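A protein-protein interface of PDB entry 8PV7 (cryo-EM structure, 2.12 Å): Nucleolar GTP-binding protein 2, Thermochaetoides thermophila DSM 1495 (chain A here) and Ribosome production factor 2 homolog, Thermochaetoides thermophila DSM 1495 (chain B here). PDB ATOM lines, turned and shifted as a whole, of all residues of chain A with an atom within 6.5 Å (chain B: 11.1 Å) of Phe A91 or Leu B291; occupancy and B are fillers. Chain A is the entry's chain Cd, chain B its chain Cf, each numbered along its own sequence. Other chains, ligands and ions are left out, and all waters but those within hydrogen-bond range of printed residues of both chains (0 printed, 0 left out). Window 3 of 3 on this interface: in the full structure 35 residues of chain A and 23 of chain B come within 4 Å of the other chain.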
ATOM      1  N   ILE A  83       0.857  -4.469  15.206  1.00  0.00           N
ATOM      2  CA  ILE A  83       0.849  -3.824  13.899  1.00  0.00           C
ATOM      3  C   ILE A  83      -0.151  -2.676  13.931  1.00  0.00           C
ATOM      4  O   ILE A  83      -1.198  -2.763  14.579  1.00  0.00           O
ATOM      5  CB  ILE A  83       0.548  -4.837  12.764  1.00  0.00           C
ATOM      6  CG1 ILE A  83       0.790  -4.215  11.388  1.00  0.00           C
ATOM      7  CG2 ILE A  83      -0.859  -5.421  12.863  1.00  0.00           C
ATOM      8  CD1 ILE A  83       0.846  -5.218  10.269  1.00  0.00           C
ATOM      9  N   ASP A  86      -2.310   1.804   9.818  1.00  0.00           N
ATOM     10  CA  ASP A  86      -1.695   2.356   8.613  1.00  0.00           C
ATOM     11  C   ASP A  86      -0.802   1.328   7.929  1.00  0.00           C
ATOM     12  O   ASP A  86      -0.797   1.212   6.695  1.00  0.00           O
ATOM     13  CB  ASP A  86      -0.894   3.606   8.965  1.00  0.00           C
ATOM     14  CG  ASP A  86      -1.624   4.510   9.928  1.00  0.00           C
ATOM     15  OD1 ASP A  86      -2.072   4.013  10.984  1.00  0.00           O
ATOM     16  OD2 ASP A  86      -1.754   5.716   9.631  1.00  0.00           O
ATOM     17  N   THR A  87      -0.039   0.575   8.723  1.00  0.00           N
ATOM     18  CA  THR A  87       0.788  -0.498   8.184  1.00  0.00           C
ATOM     19  C   THR A  87      -0.068  -1.584   7.545  1.00  0.00           C
ATOM     20  O   THR A  87       0.264  -2.093   6.466  1.00  0.00           O
ATOM     21  CB  THR A  87       1.664  -1.077   9.296  1.00  0.00           C
ATOM     22  OG1 THR A  87       2.463  -0.033   9.862  1.00  0.00           O
ATOM     23  CG2 THR A  87       2.576  -2.153   8.763  1.00  0.00           C
ATOM     24  N   LEU A  88      -1.191  -1.927   8.185  1.00  0.00           N
ATOM     25  CA  LEU A  88      -2.103  -2.910   7.605  1.00  0.00           C
ATOM     26  C   LEU A  88      -2.681  -2.420   6.283  1.00  0.00           C
ATOM     27  O   LEU A  88      -2.796  -3.194   5.328  1.00  0.00           O
ATOM     28  CB  LEU A  88      -3.227  -3.240   8.582  1.00  0.00           C
ATOM     29  CG  LEU A  88      -2.915  -4.269   9.664  1.00  0.00           C
ATOM     30  CD1 LEU A  88      -4.028  -4.309  10.690  1.00  0.00           C
ATOM     31  CD2 LEU A  88      -2.702  -5.633   9.043  1.00  0.00           C
ATOM     32  N   GLN A  89      -3.039  -1.137   6.205  1.00  0.00           N
ATOM     33  CA  GLN A  89      -3.599  -0.600   4.969  1.00  0.00           C
ATOM     34  C   GLN A  89      -2.563  -0.583   3.848  1.00  0.00           C
ATOM     35  O   GLN A  89      -2.882  -0.888   2.689  1.00  0.00           O
ATOM     36  CB  GLN A  89      -4.163   0.798   5.216  1.00  0.00           C
ATOM     37  CG  GLN A  89      -4.816   1.434   4.005  1.00  0.00           C
ATOM     38  CD  GLN A  89      -6.025   0.656   3.514  1.00  0.00           C
ATOM     39  OE1 GLN A  89      -6.748   0.039   4.298  1.00  0.00           O
ATOM     40  NE2 GLN A  89      -6.249   0.680   2.206  1.00  0.00           N
ATOM     41  N   SER A  90      -1.311  -0.254   4.180  1.00  0.00           N
ATOM     42  CA  SER A  90      -0.239  -0.305   3.189  1.00  0.00           C
ATOM     43  C   SER A  90      -0.022  -1.726   2.683  1.00  0.00           C
ATOM     44  O   SER A  90       0.195  -1.948   1.485  1.00  0.00           O
ATOM     45  CB  SER A  90       1.051   0.251   3.784  1.00  0.00           C
ATOM     46  OG  SER A  90       0.865   1.571   4.256  1.00  0.00           O
ATOM     47  N   PHE A  91      -0.095  -2.707   3.583  1.00  0.00           N
ATOM     48  CA  PHE A  91       0.094  -4.092   3.163  1.00  0.00           C
ATOM     49  C   PHE A  91      -1.085  -4.597   2.337  1.00  0.00           C
ATOM     50  O   PHE A  91      -0.909  -5.431   1.445  1.00  0.00           O
ATOM     51  CB  PHE A  91       0.327  -4.980   4.379  1.00  0.00           C
ATOM     52  CG  PHE A  91       1.734  -4.940   4.886  1.00  0.00           C
ATOM     53  CD1 PHE A  91       2.794  -4.842   4.005  1.00  0.00           C
ATOM     54  CD2 PHE A  91       1.999  -5.015   6.239  1.00  0.00           C
ATOM     55  CE1 PHE A  91       4.093  -4.812   4.467  1.00  0.00           C
ATOM     56  CE2 PHE A  91       3.294  -4.986   6.704  1.00  0.00           C
ATOM     57  CZ  PHE A  91       4.341  -4.884   5.819  1.00  0.00           C
ATOM     58  N   ARG A  92      -2.294  -4.104   2.614  1.00  0.00           N
ATOM     59  CA  ARG A  92      -3.441  -4.453   1.775  1.00  0.00           C
ATOM     60  C   ARG A  92      -3.306  -3.858   0.379  1.00  0.00           C
ATOM     61  O   ARG A  92      -3.682  -4.490  -0.616  1.00  0.00           O
ATOM     62  CB  ARG A  92      -4.739  -3.982   2.425  1.00  0.00           C
ATOM     63  CG  ARG A  92      -5.095  -4.714   3.694  1.00  0.00           C
ATOM     64  CD  ARG A  92      -6.496  -4.388   4.142  1.00  0.00           C
ATOM     65  NE  ARG A  92      -6.731  -4.807   5.517  1.00  0.00           N
ATOM     66  CZ  ARG A  92      -6.766  -3.984   6.555  1.00  0.00           C
ATOM     67  NH1 ARG A  92      -6.615  -2.680   6.410  1.00  0.00           N
ATOM     68  NH2 ARG A  92      -6.966  -4.483   7.771  1.00  0.00           N
ATOM     69  N   GLU A  93      -2.775  -2.638   0.287  1.00  0.00           N
ATOM     70  CA  GLU A  93      -2.501  -2.066  -1.027  1.00  0.00           C
ATOM     71  C   GLU A  93      -1.426  -2.862  -1.765  1.00  0.00           C
ATOM     72  O   GLU A  93      -1.499  -3.036  -2.987  1.00  0.00           O
ATOM     73  CB  GLU A  93      -2.093  -0.604  -0.881  1.00  0.00           C
ATOM     74  CG  GLU A  93      -3.268   0.349  -0.886  1.00  0.00           C
ATOM     75  CD  GLU A  93      -3.122   1.445   0.146  1.00  0.00           C
ATOM     76  OE1 GLU A  93      -1.988   1.657   0.621  1.00  0.00           O
ATOM     77  OE2 GLU A  93      -4.135   2.091   0.486  1.00  0.00           O
ATOM     78  N   ALA A  94      -0.426  -3.361  -1.036  1.00  0.00           N
ATOM     79  CA  ALA A  94       0.573  -4.230  -1.655  1.00  0.00           C
ATOM     80  C   ALA A  94      -0.050  -5.534  -2.149  1.00  0.00           C
ATOM     81  O   ALA A  94       0.298  -6.023  -3.232  1.00  0.00           O
ATOM     82  CB  ALA A  94       1.703  -4.512  -0.668  1.00  0.00           C
ATOM     83  N   MET A  95      -0.963  -6.109  -1.359  1.00  0.00           N
ATOM     84  CA  MET A  95      -1.755  -7.261  -1.790  1.00  0.00           C
ATOM     85  C   MET A  95      -2.497  -6.984  -3.090  1.00  0.00           C
ATOM     86  O   MET A  95      -2.514  -7.822  -3.999  1.00  0.00           O
ATOM     87  CB  MET A  95      -2.762  -7.639  -0.698  1.00  0.00           C
ATOM     88  CG  MET A  95      -3.217  -9.111  -0.588  1.00  0.00           C
ATOM     89  SD  MET A  95      -2.233 -10.630  -0.474  1.00  0.00           S
ATOM     90  CE  MET A  95      -0.620 -10.095   0.031  1.00  0.00           C
ATOM     91  N   ALA A  96      -3.132  -5.819  -3.187  1.00  0.00           N
ATOM     92  CA  ALA A  96      -3.937  -5.524  -4.369  1.00  0.00           C
ATOM     93  C   ALA A  96      -3.066  -5.279  -5.598  1.00  0.00           C
ATOM     94  O   ALA A  96      -3.443  -5.647  -6.715  1.00  0.00           O
ATOM     95  CB  ALA A  96      -4.849  -4.330  -4.099  1.00  0.00           C
ATOM     96  N   GLU A  97      -1.898  -4.659  -5.419  1.00  0.00           N
ATOM     97  CA  GLU A  97      -1.031  -4.374  -6.559  1.00  0.00           C
ATOM     98  C   GLU A  97       0.020  -5.446  -6.831  1.00  0.00           C
ATOM     99  O   GLU A  97       0.864  -5.237  -7.708  1.00  0.00           O
ATOM    100  CB  GLU A  97      -0.322  -3.027  -6.383  1.00  0.00           C
ATOM    101  CG  GLU A  97      -1.148  -1.789  -6.730  1.00  0.00           C
ATOM    102  CD  GLU A  97      -1.961  -1.239  -5.573  1.00  0.00           C
ATOM    103  OE1 GLU A  97      -2.909  -1.914  -5.132  1.00  0.00           O
ATOM    104  OE2 GLU A  97      -1.648  -0.125  -5.102  1.00  0.00           O
ATOM    105  N   ASN A 110       8.138 -12.845   4.827  1.00  0.00           N
ATOM    106  CA  ASN A 110       7.960 -11.863   5.884  1.00  0.00           C
ATOM    107  C   ASN A 110       6.856 -12.349   6.814  1.00  0.00           C
ATOM    108  O   ASN A 110       5.752 -12.663   6.358  1.00  0.00           O
ATOM    109  CB  ASN A 110       7.620 -10.495   5.294  1.00  0.00           C
ATOM    110  CG  ASN A 110       7.781  -9.374   6.289  1.00  0.00           C
ATOM    111  OD1 ASN A 110       8.363  -9.554   7.352  1.00  0.00           O
ATOM    112  ND2 ASN A 110       7.269  -8.203   5.946  1.00  0.00           N
ATOM    113  N   LEU A 112       3.918 -12.053   8.769  1.00  0.00           N
ATOM    114  CA  LEU A 112       2.843 -11.078   8.745  1.00  0.00           C
ATOM    115  C   LEU A 112       1.556 -11.733   9.213  1.00  0.00           C
ATOM    116  O   LEU A 112       1.398 -12.953   9.106  1.00  0.00           O
ATOM    117  CB  LEU A 112       2.646 -10.493   7.340  1.00  0.00           C
ATOM    118  CG  LEU A 112       3.671  -9.459   6.889  1.00  0.00           C
ATOM    119  CD1 LEU A 112       3.342  -8.935   5.503  1.00  0.00           C
ATOM    120  CD2 LEU A 112       3.737  -8.325   7.894  1.00  0.00           C
ATOM    121  N   PRO A 113       0.620 -10.952   9.746  1.00  0.00           N
ATOM    122  CA  PRO A 113      -0.740 -11.467   9.981  1.00  0.00           C
ATOM    123  C   PRO A 113      -1.553 -11.447   8.688  1.00  0.00           C
ATOM    124  O   PRO A 113      -2.328 -10.538   8.398  1.00  0.00           O
ATOM    125  CB  PRO A 113      -1.286 -10.503  11.036  1.00  0.00           C
ATOM    126  CG  PRO A 113      -0.572  -9.235  10.782  1.00  0.00           C
ATOM    127  CD  PRO A 113       0.790  -9.588  10.275  1.00  0.00           C
ATOM    128  N   ILE A 117      -4.649  -9.157   6.089  1.00  0.00           N
ATOM    129  CA  ILE A 117      -4.103  -8.474   4.929  1.00  0.00           C
ATOM    130  C   ILE A 117      -4.714  -8.982   3.630  1.00  0.00           C
ATOM    131  O   ILE A 117      -5.053  -8.186   2.748  1.00  0.00           O
ATOM    132  CB  ILE A 117      -2.563  -8.603   4.893  1.00  0.00           C
ATOM    133  CG1 ILE A 117      -1.956  -8.002   6.160  1.00  0.00           C
ATOM    134  CG2 ILE A 117      -1.977  -7.955   3.646  1.00  0.00           C
ATOM    135  CD1 ILE A 117      -0.485  -8.246   6.312  1.00  0.00           C
ATOM    136  N   SER B 288      16.346  -8.043  -3.454  1.00  0.00           N
ATOM    137  CA  SER B 288      15.559  -6.865  -3.134  1.00  0.00           C
ATOM    138  C   SER B 288      14.492  -7.244  -2.121  1.00  0.00           C
ATOM    139  O   SER B 288      14.367  -8.399  -1.718  1.00  0.00           O
ATOM    140  CB  SER B 288      14.935  -6.246  -4.387  1.00  0.00           C
ATOM    141  OG  SER B 288      13.940  -7.089  -4.931  1.00  0.00           O
ATOM    142  N   MET B 289      13.728  -6.244  -1.705  1.00  0.00           N
ATOM    143  CA  MET B 289      12.606  -6.421  -0.798  1.00  0.00           C
ATOM    144  C   MET B 289      11.344  -5.952  -1.502  1.00  0.00           C
ATOM    145  O   MET B 289      11.309  -4.839  -2.034  1.00  0.00           O
ATOM    146  CB  MET B 289      12.823  -5.628   0.490  1.00  0.00           C
ATOM    147  CG  MET B 289      11.946  -6.051   1.641  1.00  0.00           C
ATOM    148  SD  MET B 289      12.349  -5.137   3.133  1.00  0.00           S
ATOM    149  CE  MET B 289      10.993  -3.975   3.195  1.00  0.00           C
ATOM    150  N   ASP B 290      10.314  -6.790  -1.513  1.00  0.00           N
ATOM    151  CA  ASP B 290       9.105  -6.387  -2.214  1.00  0.00           C
ATOM    152  C   ASP B 290       8.238  -5.507  -1.311  1.00  0.00           C
ATOM    153  O   ASP B 290       8.625  -5.134  -0.201  1.00  0.00           O
ATOM    154  CB  ASP B 290       8.356  -7.609  -2.749  1.00  0.00           C
ATOM    155  CG  ASP B 290       7.757  -8.480  -1.660  1.00  0.00           C
ATOM    156  OD1 ASP B 290       8.107  -8.326  -0.476  1.00  0.00           O
ATOM    157  OD2 ASP B 290       6.912  -9.332  -2.000  1.00  0.00           O
ATOM    158  N   LEU B 291       7.038  -5.177  -1.788  1.00  0.00           N
ATOM    159  CA  LEU B 291       6.166  -4.285  -1.036  1.00  0.00           C
ATOM    160  C   LEU B 291       5.548  -4.961   0.180  1.00  0.00           C
ATOM    161  O   LEU B 291       5.010  -4.269   1.049  1.00  0.00           O
ATOM    162  CB  LEU B 291       5.071  -3.740  -1.945  1.00  0.00           C
ATOM    163  CG  LEU B 291       5.544  -2.711  -2.969  1.00  0.00           C
ATOM    164  CD1 LEU B 291       4.387  -2.263  -3.840  1.00  0.00           C
ATOM    165  CD2 LEU B 291       6.189  -1.531  -2.273  1.00  0.00           C
ATOM    166  N   LEU B 292       5.612  -6.286   0.259  1.00  0.00           N
ATOM    167  CA  LEU B 292       5.153  -7.036   1.418  1.00  0.00           C
ATOM    168  C   LEU B 292       6.265  -7.311   2.415  1.00  0.00           C
ATOM    169  O   LEU B 292       6.005  -7.892   3.470  1.00  0.00           O
ATOM    170  CB  LEU B 292       4.547  -8.358   0.972  1.00  0.00           C
ATOM    171  CG  LEU B 292       3.186  -8.283   0.303  1.00  0.00           C
ATOM    172  CD1 LEU B 292       2.919  -9.599  -0.387  1.00  0.00           C
ATOM    173  CD2 LEU B 292       2.122  -7.965   1.335  1.00  0.00           C
ATOM    174  N   GLY B 293       7.493  -6.923   2.103  1.00  0.00           N
ATOM    175  CA  GLY B 293       8.619  -7.220   2.955  1.00  0.00           C
ATOM    176  C   GLY B 293       9.288  -8.552   2.714  1.00  0.00           C
ATOM    177  O   GLY B 293      10.221  -8.893   3.448  1.00  0.00           O
ATOM    178  N   ASP B 294       8.836  -9.326   1.733  1.00  0.00           N
ATOM    179  CA  ASP B 294       9.515 -10.560   1.371  1.00  0.00           C
ATOM    180  C   ASP B 294      10.837 -10.253   0.683  1.00  0.00           C
ATOM    181  O   ASP B 294      10.951  -9.297  -0.091  1.00  0.00           O
ATOM    182  CB  ASP B 294       8.648 -11.408   0.440  1.00  0.00           C
ATOM    183  CG  ASP B 294       7.327 -11.796   1.060  1.00  0.00           C
ATOM    184  OD1 ASP B 294       7.206 -11.753   2.299  1.00  0.00           O
ATOM    185  OD2 ASP B 294       6.398 -12.143   0.303  1.00  0.00           O
ATOM    186  N   LYS B 295      11.838 -11.079   0.968  1.00  0.00           N
ATOM    187  CA  LYS B 295      13.110 -10.990   0.270  1.00  0.00           C
ATOM    188  C   LYS B 295      12.998 -11.727  -1.056  1.00  0.00           C
ATOM    189  O   LYS B 295      12.618 -12.899  -1.094  1.00  0.00           O
ATOM    190  CB  LYS B 295      14.235 -11.578   1.117  1.00  0.00           C
ATOM    191  CG  LYS B 295      15.613 -11.360   0.533  1.00  0.00           C
ATOM    192  CD  LYS B 295      16.686 -12.022   1.373  1.00  0.00           C
ATOM    193  CE  LYS B 295      16.765 -11.417   2.756  1.00  0.00           C
ATOM    194  NZ  LYS B 295      17.778 -12.116   3.587  1.00  0.00           N
ATOM    195  N   ILE B 296      13.314 -11.033  -2.142  1.00  0.00           N
ATOM    196  CA  ILE B 296      13.097 -11.523  -3.494  1.00  0.00           C
ATOM    197  C   ILE B 296      14.435 -11.594  -4.213  1.00  0.00           C
ATOM    198  O   ILE B 296      15.214 -10.636  -4.193  1.00  0.00           O
ATOM    199  CB  ILE B 296      12.115 -10.619  -4.266  1.00  0.00           C
ATOM    200  CG1 ILE B 296      10.823 -10.427  -3.474  1.00  0.00           C
ATOM    201  CG2 ILE B 296      11.812 -11.198  -5.616  1.00  0.00           C
ATOM    202  CD1 ILE B 296      10.090 -11.711  -3.186  1.00  0.00           C
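The backbone carbonyl oxygen (O) of Leu B292 is in hydrogen-bond range of the side-chain amide nitrogen (ND2) of Asn A110, 2.8 Å away. OD1 of Asp B294 is in hydrogen-bond range of N of Asn A110, at 2.9 Å.
The backbone NH (N) of Leu B292 sits close to the side-chain carboxylate (OD1) of Asp B290. OD1 of Asp B290 sits at hydrogen-bond distance from N of Asp B294. N of Gly B293 is in hydrogen-bond range of OD1 of Asp B290 (3.0 Å).
Among the printed residues, pairs that only touch across the chains: Phe A91 with Leu B291, Phe A91 with Leu B292, Ala A94 with Leu B291, Met A95 with Leu B292, Asn A110 with Gly B293 and Leu A112 with Leu B292.
Printed residues of chain B within 4 Å of Phe A91: Leu B291 (3.6 Å) and Leu B292 (3.8 Å). Leu B291 touches two residues of chain A. Thr A87 touches none of the printed residues of chain B. No residue of chain B comes within 4 Å of Ser A90. Glu A93 touches none of the printed residues of chain B. Met A95 touches just one residue of chain B: Leu B292 (3.6 Å). No residue of chain B comes within 4 Å of Ile A117. Of the printed residues of chain A, Gly B293 touches Asn A110. Printed residues of chain B within 4 Å of Leu A112: Leu B292. Printed residues of chain A within 4 Å of Asp B294: Asn A110. Printed residues of chain B within 4 Å of Asn A110: Leu B292, Gly B293 and Asp B294. Of the printed residues of chain A, Leu B292 touches Phe A91, Met A95, Asn A110 and Leu A112. The nearest residue of chain B that does not touch Phe A91 is Gly B293 (4.6 Å). The nearest residue of chain A that does not touch Leu B291 is Ser A90 (5.4 Å). The nearest printed residue of chain A that does not touch Leu B292 is Ala A94 (4.01 Å).
Of the 17 printed residues of chain A, 5 touch a printed residue of chain B. Hydrophobic or aromatic side chains of chain A that line the printed part of chain B: Phe A91, Ala A94, Met A95 and Leu A112. Along chain A the printed residues that touch a printed residue of chain B span positions 91 to 112. Of the 9 printed residues of chain B, 4 touch a printed residue of chain A. Printed residues of chain B that touch a printed residue of chain A: Leu B291, Leu B292, Gly B293 and Asp B294. Hydrophobic or aromatic side chains of chain B that line the printed part of chain A: Leu B291 and Leu B292. Among the printed residues, 8 pairs touch across the chains.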
